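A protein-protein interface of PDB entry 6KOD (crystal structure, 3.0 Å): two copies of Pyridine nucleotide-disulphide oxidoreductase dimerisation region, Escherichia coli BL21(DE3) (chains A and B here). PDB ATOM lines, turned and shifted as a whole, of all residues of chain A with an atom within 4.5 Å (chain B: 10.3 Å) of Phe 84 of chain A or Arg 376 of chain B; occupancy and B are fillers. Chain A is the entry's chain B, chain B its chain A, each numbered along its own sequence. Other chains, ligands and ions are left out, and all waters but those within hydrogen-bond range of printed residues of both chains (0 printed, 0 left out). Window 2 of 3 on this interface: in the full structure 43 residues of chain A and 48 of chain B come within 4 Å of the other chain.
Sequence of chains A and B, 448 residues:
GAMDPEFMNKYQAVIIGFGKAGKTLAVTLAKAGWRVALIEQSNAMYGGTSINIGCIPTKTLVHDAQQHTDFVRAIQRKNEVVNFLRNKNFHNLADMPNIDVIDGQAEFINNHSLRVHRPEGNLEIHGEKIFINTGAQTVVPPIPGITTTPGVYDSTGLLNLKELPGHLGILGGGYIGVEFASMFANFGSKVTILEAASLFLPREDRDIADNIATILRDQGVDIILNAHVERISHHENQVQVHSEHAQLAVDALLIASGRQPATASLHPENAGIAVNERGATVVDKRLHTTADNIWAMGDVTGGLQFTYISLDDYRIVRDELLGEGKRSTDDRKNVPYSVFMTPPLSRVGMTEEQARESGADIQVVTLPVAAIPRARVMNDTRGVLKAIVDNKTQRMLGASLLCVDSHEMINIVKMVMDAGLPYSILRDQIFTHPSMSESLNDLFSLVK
Of the 22 printed residues of chain B, 4 touch a printed residue of chain A. Along chain B the printed residues that touch a printed residue of chain A span positions 373 to 379. Printed residues of chain A that touch a printed residue of chain B: Arg 77, Val 81, Phe 84 and Leu 85. Hydrophobic or aromatic side chains of chain A that line the printed part of chain B: Val 81, Phe 84 and Leu 85. Among the printed residues, no Asp or Glu carboxylate lies within 4 Å of a Lys or Arg side-chain nitrogen of the other chain.
NH1 of Arg 376 of chain B sits at hydrogen-bond distance from O of Ala 370 of chain B (2.9 Å).
The backbone carbonyl oxygen (O) of Val 377 of chain B sits at hydrogen-bond distance from the guanidinium group (NH2) of Arg 77 of chain A (2.9 Å). OD1 of Asn 379 of chain B sits at hydrogen-bond distance from NE of Arg 77 of chain A, 3.4 Å away. O of Arg 376 of chain B sits close to NH2 of Arg 77 of chain A, at 2.3 Å.
CG1 of Val 81 of chain A touches CB of Arg 376 of chain B, at 3.8 Å. Phe 84 of chain A touches Arg 376 of chain B (CE2 to CZ, 3.2 Å). Leu 85 of chain A touches Pro 373 of chain B (CD1 to CB, 3.9 Å).
Printed residues of chain B within 4 Å of Arg 77 of chain A: Arg 376 (2.3 Å), Val 377 (2.9 Å) and Asn 379 (3.3 Å). Val 81 of chain A touches one residue of chain B. No residue of chain B comes within 4 Å of Asn 83 of chain A. Phe 84 of chain A touches just one residue of chain B: Arg 376 (3.2 Å). Of the printed residues of chain A, Pro 373 of chain B touches Leu 85 (3.9 Å). Of the printed residues of chain A, Val 377 of chain B touches Arg 77. Of the printed residues of chain A, Asn 379 of chain B touches Arg 77. Val 404 of chain B touches none of the printed residues of chain A.
No position is printed for both chains.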
ATOM      1  N   ARG A  77      -1.158 -32.059   0.450  1.00  0.00           N
ATOM      2  CA  ARG A  77      -1.810 -31.087   1.322  1.00  0.00           C
ATOM      3  C   ARG A  77      -1.385 -29.666   0.976  1.00  0.00           C
ATOM      4  O   ARG A  77      -2.166 -28.722   1.146  1.00  0.00           O
ATOM      5  CB  ARG A  77      -1.504 -31.392   2.789  1.00  0.00           C
ATOM      6  CG  ARG A  77      -2.427 -30.681   3.770  1.00  0.00           C
ATOM      7  CD  ARG A  77      -1.670 -30.177   4.988  1.00  0.00           C
ATOM      8  NE  ARG A  77      -2.110 -28.847   5.404  1.00  0.00           N
ATOM      9  CZ  ARG A  77      -1.391 -28.025   6.162  1.00  0.00           C
ATOM     10  NH1 ARG A  77      -0.189 -28.392   6.590  1.00  0.00           N
ATOM     11  NH2 ARG A  77      -1.869 -26.834   6.489  1.00  0.00           N
ATOM     12  N   GLU A  80      -3.487 -28.948  -1.950  1.00  0.00           N
ATOM     13  CA  GLU A  80      -4.876 -28.685  -1.590  1.00  0.00           C
ATOM     14  C   GLU A  80      -5.069 -27.233  -1.172  1.00  0.00           C
ATOM     15  O   GLU A  80      -6.078 -26.610  -1.523  1.00  0.00           O
ATOM     16  CB  GLU A  80      -5.322 -29.637  -0.484  1.00  0.00           C
ATOM     17  CG  GLU A  80      -5.522 -31.066  -0.961  1.00  0.00           C
ATOM     18  CD  GLU A  80      -5.938 -32.000   0.156  1.00  0.00           C
ATOM     19  OE1 GLU A  80      -5.633 -31.699   1.329  1.00  0.00           O
ATOM     20  OE2 GLU A  80      -6.572 -33.035  -0.140  1.00  0.00           O
ATOM     21  N   VAL A  81      -4.106 -26.670  -0.440  1.00  0.00           N
ATOM     22  CA  VAL A  81      -4.232 -25.291   0.020  1.00  0.00           C
ATOM     23  C   VAL A  81      -3.967 -24.312  -1.116  1.00  0.00           C
ATOM     24  O   VAL A  81      -4.692 -23.324  -1.279  1.00  0.00           O
ATOM     25  CB  VAL A  81      -3.292 -25.042   1.214  1.00  0.00           C
ATOM     26  CG1 VAL A  81      -3.047 -23.550   1.403  1.00  0.00           C
ATOM     27  CG2 VAL A  81      -3.872 -25.655   2.478  1.00  0.00           C
ATOM     28  N   VAL A  82      -2.938 -24.571  -1.925  1.00  0.00           N
ATOM     29  CA  VAL A  82      -2.556 -23.626  -2.970  1.00  0.00           C
ATOM     30  C   VAL A  82      -3.610 -23.586  -4.071  1.00  0.00           C
ATOM     31  O   VAL A  82      -4.018 -22.508  -4.521  1.00  0.00           O
ATOM     32  CB  VAL A  82      -1.165 -23.976  -3.529  1.00  0.00           C
ATOM     33  CG1 VAL A  82      -0.954 -23.319  -4.884  1.00  0.00           C
ATOM     34  CG2 VAL A  82      -0.083 -23.548  -2.554  1.00  0.00           C
ATOM     35  N   ASN A  83      -4.068 -24.758  -4.523  1.00  0.00           N
ATOM     36  CA  ASN A  83      -5.112 -24.792  -5.543  1.00  0.00           C
ATOM     37  C   ASN A  83      -6.405 -24.159  -5.045  1.00  0.00           C
ATOM     38  O   ASN A  83      -7.169 -23.600  -5.842  1.00  0.00           O
ATOM     39  CB  ASN A  83      -5.354 -26.230  -6.010  1.00  0.00           C
ATOM     40  CG  ASN A  83      -4.102 -26.874  -6.589  1.00  0.00           C
ATOM     41  OD1 ASN A  83      -2.989 -26.634  -6.116  1.00  0.00           O
ATOM     42  ND2 ASN A  83      -4.280 -27.691  -7.623  1.00  0.00           N
ATOM     43  N   PHE A  84      -6.658 -24.213  -3.735  1.00  0.00           N
ATOM     44  CA  PHE A  84      -7.830 -23.540  -3.182  1.00  0.00           C
ATOM     45  C   PHE A  84      -7.640 -22.028  -3.173  1.00  0.00           C
ATOM     46  O   PHE A  84      -8.514 -21.279  -3.622  1.00  0.00           O
ATOM     47  CB  PHE A  84      -8.120 -24.050  -1.769  1.00  0.00           C
ATOM     48  CG  PHE A  84      -9.238 -23.315  -1.080  1.00  0.00           C
ATOM     49  CD1 PHE A  84     -10.553 -23.709  -1.255  1.00  0.00           C
ATOM     50  CD2 PHE A  84      -8.975 -22.224  -0.263  1.00  0.00           C
ATOM     51  CE1 PHE A  84     -11.586 -23.032  -0.628  1.00  0.00           C
ATOM     52  CE2 PHE A  84     -10.003 -21.541   0.361  1.00  0.00           C
ATOM     53  CZ  PHE A  84     -11.309 -21.947   0.180  1.00  0.00           C
ATOM     54  N   LEU A  85      -6.500 -21.563  -2.657  1.00  0.00           N
ATOM     55  CA  LEU A  85      -6.266 -20.128  -2.541  1.00  0.00           C
ATOM     56  C   LEU A  85      -5.979 -19.472  -3.886  1.00  0.00           C
ATOM     57  O   LEU A  85      -6.202 -18.265  -4.029  1.00  0.00           O
ATOM     58  CB  LEU A  85      -5.114 -19.861  -1.573  1.00  0.00           C
ATOM     59  CG  LEU A  85      -5.489 -19.693  -0.101  1.00  0.00           C
ATOM     60  CD1 LEU A  85      -4.270 -19.305   0.719  1.00  0.00           C
ATOM     61  CD2 LEU A  85      -6.598 -18.664   0.063  1.00  0.00           C
ATOM     62  N   ARG A  86      -5.488 -20.232  -4.868  1.00  0.00           N
ATOM     63  CA  ARG A  86      -5.290 -19.667  -6.199  1.00  0.00           C
ATOM     64  C   ARG A  86      -6.623 -19.325  -6.851  1.00  0.00           C
ATOM     65  O   ARG A  86      -6.767 -18.260  -7.463  1.00  0.00           O
ATOM     66  CB  ARG A  86      -4.501 -20.641  -7.076  1.00  0.00           C
ATOM     67  CG  ARG A  86      -4.278 -20.152  -8.504  1.00  0.00           C
ATOM     68  CD  ARG A  86      -3.793 -21.274  -9.417  1.00  0.00           C
ATOM     69  NE  ARG A  86      -2.550 -21.875  -8.940  1.00  0.00           N
ATOM     70  CZ  ARG A  86      -2.158 -23.113  -9.226  1.00  0.00           C
ATOM     71  NH1 ARG A  86      -2.913 -23.891  -9.990  1.00  0.00           N
ATOM     72  NH2 ARG A  86      -1.010 -23.576  -8.747  1.00  0.00           N
ATOM     73  N   ASN A  87      -7.611 -20.214  -6.726  1.00  0.00           N
ATOM     74  CA  ASN A  87      -8.914 -19.957  -7.327  1.00  0.00           C
ATOM     75  C   ASN A  87      -9.663 -18.854  -6.592  1.00  0.00           C
ATOM     76  O   ASN A  87     -10.384 -18.072  -7.222  1.00  0.00           O
ATOM     77  CB  ASN A  87      -9.742 -21.242  -7.356  1.00  0.00           C
ATOM     78  CG  ASN A  87      -9.198 -22.262  -8.339  1.00  0.00           C
ATOM     79  OD1 ASN A  87      -8.802 -21.919  -9.453  1.00  0.00           O
ATOM     80  ND2 ASN A  87      -9.177 -23.525  -7.929  1.00  0.00           N
ATOM     81  N   LYS A  88      -9.504 -18.771  -5.269  1.00  0.00           N
ATOM     82  CA  LYS A  88     -10.156 -17.704  -4.514  1.00  0.00           C
ATOM     83  C   LYS A  88      -9.581 -16.343  -4.881  1.00  0.00           C
ATOM     84  O   LYS A  88     -10.323 -15.362  -5.006  1.00  0.00           O
ATOM     85  CB  LYS A  88     -10.017 -17.958  -3.014  1.00  0.00           C
ATOM     86  CG  LYS A  88     -10.668 -16.896  -2.138  1.00  0.00           C
ATOM     87  CD  LYS A  88     -12.150 -17.174  -1.940  1.00  0.00           C
ATOM     88  CE  LYS A  88     -12.806 -16.105  -1.078  1.00  0.00           C
ATOM     89  NZ  LYS A  88     -13.298 -14.955  -1.887  1.00  0.00           N
ATOM     90  N   PRO B 368     -13.650 -13.803   9.419  1.00  0.00           N
ATOM     91  CA  PRO B 368     -13.538 -15.248   9.648  1.00  0.00           C
ATOM     92  C   PRO B 368     -12.117 -15.733   9.399  1.00  0.00           C
ATOM     93  O   PRO B 368     -11.385 -15.195   8.564  1.00  0.00           O
ATOM     94  CB  PRO B 368     -14.526 -15.851   8.640  1.00  0.00           C
ATOM     95  CG  PRO B 368     -14.785 -14.765   7.642  1.00  0.00           C
ATOM     96  CD  PRO B 368     -14.646 -13.477   8.386  1.00  0.00           C
ATOM     97  N   VAL B 369     -11.727 -16.766  10.151  1.00  0.00           N
ATOM     98  CA  VAL B 369     -10.367 -17.283  10.067  1.00  0.00           C
ATOM     99  C   VAL B 369     -10.084 -17.914   8.708  1.00  0.00           C
ATOM    100  O   VAL B 369      -8.923 -17.965   8.283  1.00  0.00           O
ATOM    101  CB  VAL B 369     -10.124 -18.278  11.221  1.00  0.00           C
ATOM    102  CG1 VAL B 369      -8.715 -18.832  11.181  1.00  0.00           C
ATOM    103  CG2 VAL B 369     -10.363 -17.593  12.551  1.00  0.00           C
ATOM    104  N   ALA B 370     -11.120 -18.368   7.998  1.00  0.00           N
ATOM    105  CA  ALA B 370     -10.919 -18.966   6.683  1.00  0.00           C
ATOM    106  C   ALA B 370     -10.242 -18.012   5.706  1.00  0.00           C
ATOM    107  O   ALA B 370      -9.661 -18.469   4.716  1.00  0.00           O
ATOM    108  CB  ALA B 370     -12.255 -19.434   6.108  1.00  0.00           C
ATOM    109  N   ALA B 371     -10.297 -16.706   5.962  1.00  0.00           N
ATOM    110  CA  ALA B 371      -9.651 -15.713   5.116  1.00  0.00           C
ATOM    111  C   ALA B 371      -8.198 -15.458   5.499  1.00  0.00           C
ATOM    112  O   ALA B 371      -7.524 -14.674   4.823  1.00  0.00           O
ATOM    113  CB  ALA B 371     -10.432 -14.395   5.159  1.00  0.00           C
ATOM    114  N   ILE B 372      -7.703 -16.092   6.559  1.00  0.00           N
ATOM    115  CA  ILE B 372      -6.316 -15.941   6.989  1.00  0.00           C
ATOM    116  C   ILE B 372      -5.502 -17.055   6.333  1.00  0.00           C
ATOM    117  O   ILE B 372      -5.673 -18.228   6.706  1.00  0.00           O
ATOM    118  CB  ILE B 372      -6.189 -15.990   8.517  1.00  0.00           C
ATOM    119  CG1 ILE B 372      -6.920 -14.805   9.154  1.00  0.00           C
ATOM    120  CG2 ILE B 372      -4.722 -16.000   8.926  1.00  0.00           C
ATOM    121  CD1 ILE B 372      -7.220 -14.989  10.627  1.00  0.00           C
ATOM    122  N   PRO B 373      -4.627 -16.746   5.372  1.00  0.00           N
ATOM    123  CA  PRO B 373      -3.847 -17.816   4.725  1.00  0.00           C
ATOM    124  C   PRO B 373      -2.969 -18.591   5.690  1.00  0.00           C
ATOM    125  O   PRO B 373      -2.757 -19.794   5.490  1.00  0.00           O
ATOM    126  CB  PRO B 373      -3.009 -17.060   3.683  1.00  0.00           C
ATOM    127  CG  PRO B 373      -3.725 -15.757   3.477  1.00  0.00           C
ATOM    128  CD  PRO B 373      -4.344 -15.421   4.798  1.00  0.00           C
ATOM    129  N   ARG B 374      -2.457 -17.940   6.738  1.00  0.00           N
ATOM    130  CA  ARG B 374      -1.632 -18.643   7.714  1.00  0.00           C
ATOM    131  C   ARG B 374      -2.415 -19.743   8.420  1.00  0.00           C
ATOM    132  O   ARG B 374      -1.835 -20.759   8.819  1.00  0.00           O
ATOM    133  CB  ARG B 374      -1.061 -17.648   8.726  1.00  0.00           C
ATOM    134  CG  ARG B 374      -0.299 -18.280   9.880  1.00  0.00           C
ATOM    135  CD  ARG B 374       1.003 -18.909   9.415  1.00  0.00           C
ATOM    136  NE  ARG B 374       1.668 -19.631  10.495  1.00  0.00           N
ATOM    137  CZ  ARG B 374       2.970 -19.894  10.531  1.00  0.00           C
ATOM    138  NH1 ARG B 374       3.485 -20.556  11.557  1.00  0.00           N
ATOM    139  NH2 ARG B 374       3.759 -19.497   9.540  1.00  0.00           N
ATOM    140  N   ALA B 375      -3.730 -19.567   8.573  1.00  0.00           N
ATOM    141  CA  ALA B 375      -4.544 -20.611   9.183  1.00  0.00           C
ATOM    142  C   ALA B 375      -4.539 -21.883   8.347  1.00  0.00           C
ATOM    143  O   ALA B 375      -4.586 -22.988   8.899  1.00  0.00           O
ATOM    144  CB  ALA B 375      -5.973 -20.115   9.385  1.00  0.00           C
ATOM    145  N   ARG B 376      -4.483 -21.749   7.019  1.00  0.00           N
ATOM    146  CA  ARG B 376      -4.375 -22.928   6.168  1.00  0.00           C
ATOM    147  C   ARG B 376      -3.000 -23.571   6.280  1.00  0.00           C
ATOM    148  O   ARG B 376      -2.881 -24.796   6.163  1.00  0.00           O
ATOM    149  CB  ARG B 376      -4.667 -22.562   4.714  1.00  0.00           C
ATOM    150  CG  ARG B 376      -6.087 -22.107   4.467  1.00  0.00           C
ATOM    151  CD  ARG B 376      -6.580 -22.567   3.110  1.00  0.00           C
ATOM    152  NE  ARG B 376      -7.943 -23.083   3.177  1.00  0.00           N
ATOM    153  CZ  ARG B 376      -9.021 -22.323   3.340  1.00  0.00           C
ATOM    154  NH1 ARG B 376      -8.895 -21.006   3.443  1.00  0.00           N
ATOM    155  NH2 ARG B 376     -10.225 -22.876   3.390  1.00  0.00           N
ATOM    156  N   VAL B 377      -1.957 -22.767   6.495  1.00  0.00           N
ATOM    157  CA  VAL B 377      -0.620 -23.318   6.692  1.00  0.00           C
ATOM    158  C   VAL B 377      -0.588 -24.183   7.947  1.00  0.00           C
ATOM    159  O   VAL B 377       0.021 -25.260   7.964  1.00  0.00           O
ATOM    160  CB  VAL B 377       0.420 -22.182   6.752  1.00  0.00           C
ATOM    161  CG1 VAL B 377       1.695 -22.641   7.453  1.00  0.00           C
ATOM    162  CG2 VAL B 377       0.725 -21.663   5.358  1.00  0.00           C
ATOM    163  N   MET B 378      -1.264 -23.740   9.006  1.00  0.00           N
ATOM    164  CA  MET B 378      -1.317 -24.468  10.265  1.00  0.00           C
ATOM    165  C   MET B 378      -2.434 -25.503  10.317  1.00  0.00           C
ATOM    166  O   MET B 378      -2.580 -26.180  11.340  1.00  0.00           O
ATOM    167  CB  MET B 378      -1.477 -23.488  11.431  1.00  0.00           C
ATOM    168  CG  MET B 378      -0.560 -22.282  11.355  1.00  0.00           C
ATOM    169  SD  MET B 378       0.159 -21.868  12.954  1.00  0.00           S
ATOM    170  CE  MET B 378       1.593 -22.944  12.968  1.00  0.00           C
ATOM    171  N   ASN B 379      -3.225 -25.634   9.250  1.00  0.00           N
ATOM    172  CA  ASN B 379      -4.288 -26.640   9.162  1.00  0.00           C
ATOM    173  C   ASN B 379      -5.318 -26.470  10.279  1.00  0.00           C
ATOM    174  O   ASN B 379      -5.693 -27.425  10.963  1.00  0.00           O
ATOM    175  CB  ASN B 379      -3.707 -28.058   9.164  1.00  0.00           C
ATOM    176  CG  ASN B 379      -4.635 -29.066   8.513  1.00  0.00           C
ATOM    177  OD1 ASN B 379      -4.940 -28.967   7.324  1.00  0.00           O
ATOM    178  ND2 ASN B 379      -5.091 -30.040   9.291  1.00  0.00           N
ATOM    179  N   ASP B 380      -5.782 -25.231  10.458  1.00  0.00           N
ATOM    180  CA  ASP B 380      -6.856 -24.949  11.415  1.00  0.00           C
ATOM    181  C   ASP B 380      -7.470 -23.600  11.023  1.00  0.00           C
ATOM    182  O   ASP B 380      -7.070 -22.555  11.536  1.00  0.00           O
ATOM    183  CB  ASP B 380      -6.358 -24.939  12.848  1.00  0.00           C
ATOM    184  CG  ASP B 380      -7.480 -25.131  13.858  1.00  0.00           C
ATOM    185  OD1 ASP B 380      -7.291 -24.772  15.041  1.00  0.00           O
ATOM    186  OD2 ASP B 380      -8.553 -25.641  13.469  1.00  0.00           O
ATOM    187  N   THR B 381      -8.437 -23.648  10.107  1.00  0.00           N
ATOM    188  CA  THR B 381      -9.164 -22.464   9.669  1.00  0.00           C
ATOM    189  C   THR B 381     -10.403 -22.189  10.517  1.00  0.00           C
ATOM    190  O   THR B 381     -11.241 -21.374  10.122  1.00  0.00           O
ATOM    191  CB  THR B 381      -9.563 -22.599   8.193  1.00  0.00           C
ATOM    192  OG1 THR B 381     -10.147 -23.886   7.965  1.00  0.00           O
ATOM    193  CG2 THR B 381      -8.345 -22.447   7.298  1.00  0.00           C
ATOM    194  N   ARG B 382     -10.528 -22.843  11.670  1.00  0.00           N
ATOM    195  CA  ARG B 382     -11.669 -22.650  12.548  1.00  0.00           C
ATOM    196  C   ARG B 382     -11.530 -21.359  13.349  1.00  0.00           C
ATOM    197  O   ARG B 382     -10.437 -20.810  13.515  1.00  0.00           O
ATOM    198  CB  ARG B 382     -11.818 -23.831  13.509  1.00  0.00           C
ATOM    199  CG  ARG B 382     -12.176 -25.145  12.846  1.00  0.00           C
ATOM    200  CD  ARG B 382     -12.200 -26.267  13.864  1.00  0.00           C
ATOM    201  NE  ARG B 382     -10.931 -26.380  14.577  1.00  0.00           N
ATOM    202  CZ  ARG B 382     -10.712 -27.225  15.580  1.00  0.00           C
ATOM    203  NH1 ARG B 382     -11.677 -28.035  15.994  1.00  0.00           N
ATOM    204  NH2 ARG B 382      -9.525 -27.260  16.171  1.00  0.00           N
ATOM    205  N   CYS B 403      -8.676 -18.161  17.335  1.00  0.00           N
ATOM    206  CA  CYS B 403      -7.874 -18.704  16.246  1.00  0.00           C
ATOM    207  C   CYS B 403      -6.613 -19.322  16.831  1.00  0.00           C
ATOM    208  O   CYS B 403      -6.319 -19.174  18.019  1.00  0.00           O
ATOM    209  CB  CYS B 403      -7.517 -17.622  15.225  1.00  0.00           C
ATOM    210  SG  CYS B 403      -6.642 -16.215  15.948  1.00  0.00           S
ATOM    211  N   VAL B 404      -5.866 -20.016  15.971  1.00  0.00           N
ATOM    212  CA  VAL B 404      -4.577 -20.565  16.367  1.00  0.00           C
ATOM    213  C   VAL B 404      -3.612 -19.423  16.655  1.00  0.00           C
ATOM    214  O   VAL B 404      -3.652 -18.370  16.002  1.00  0.00           O
ATOM    215  CB  VAL B 404      -4.038 -21.507  15.274  1.00  0.00           C
ATOM    216  CG1 VAL B 404      -3.888 -20.771  13.945  1.00  0.00           C
ATOM    217  CG2 VAL B 404      -2.718 -22.144  15.702  1.00  0.00           C
ATOM    218  N   PRO B 434       4.546 -15.488   6.253  1.00  0.00           N
ATOM    219  CA  PRO B 434       3.154 -15.612   6.696  1.00  0.00           C
ATOM    220  C   PRO B 434       3.064 -15.761   8.210  1.00  0.00           C
ATOM    221  O   PRO B 434       3.913 -16.419   8.810  1.00  0.00           O
ATOM    222  CB  PRO B 434       2.662 -16.887   5.992  1.00  0.00           C
ATOM    223  CG  PRO B 434       3.827 -17.388   5.161  1.00  0.00           C
ATOM    224  CD  PRO B 434       5.057 -16.765   5.734  1.00  0.00           C
ATOM    225  N   SER B 435       2.048 -15.157   8.818  1.00  0.00           N
ATOM    226  CA  SER B 435       1.900 -15.210  10.264  1.00  0.00           C
ATOM    227  C   SER B 435       0.438 -14.985  10.615  1.00  0.00           C
ATOM    228  O   SER B 435      -0.390 -14.676   9.755  1.00  0.00           O
ATOM    229  CB  SER B 435       2.795 -14.174  10.955  1.00  0.00           C
ATOM    230  OG  SER B 435       2.412 -12.855  10.602  1.00  0.00           O
ATOM    231  N   MET B 436       0.133 -15.154  11.901  1.00  0.00           N
ATOM    232  CA  MET B 436      -1.199 -14.881  12.419  1.00  0.00           C
ATOM    233  C   MET B 436      -1.383 -13.422  12.809  1.00  0.00           C
ATOM    234  O   MET B 436      -2.486 -12.884  12.658  1.00  0.00           O
ATOM    235  CB  MET B 436      -1.482 -15.773  13.631  1.00  0.00           C
ATOM    236  CG  MET B 436      -2.829 -16.460  13.594  1.00  0.00           C
ATOM    237  SD  MET B 436      -3.116 -17.354  12.060  1.00  0.00           S
ATOM    238  CE  MET B 436      -4.885 -17.622  12.165  1.00  0.00           C
ATOM    239  N   GLU B 438      -0.444 -10.867  11.313  1.00  0.00           N
ATOM    240  CA  GLU B 438      -0.690 -10.029  10.147  1.00  0.00           C
ATOM    241  C   GLU B 438      -2.156  -9.989   9.739  1.00  0.00           C
ATOM    242  O   GLU B 438      -2.518  -9.165   8.893  1.00  0.00           O
ATOM    243  CB  GLU B 438       0.162 -10.506   8.971  1.00  0.00           C
ATOM    244  CG  GLU B 438      -0.398 -11.709   8.247  1.00  0.00           C
ATOM    245  CD  GLU B 438       0.538 -12.220   7.176  1.00  0.00           C
ATOM    246  OE1 GLU B 438       0.819 -13.435   7.168  1.00  0.00           O
ATOM    247  OE2 GLU B 438       0.994 -11.404   6.345  1.00  0.00           O
ATOM    248  N   SER B 439      -3.006 -10.848  10.307  1.00  0.00           N
ATOM    249  CA  SER B 439      -4.436 -10.741  10.042  1.00  0.00           C
ATOM    250  C   SER B 439      -5.022  -9.456  10.607  1.00  0.00           C
ATOM    251  O   SER B 439      -6.108  -9.045  10.182  1.00  0.00           O
ATOM    252  CB  SER B 439      -5.180 -11.948  10.614  1.00  0.00           C
ATOM    253  OG  SER B 439      -4.301 -12.793  11.335  1.00  0.00           O
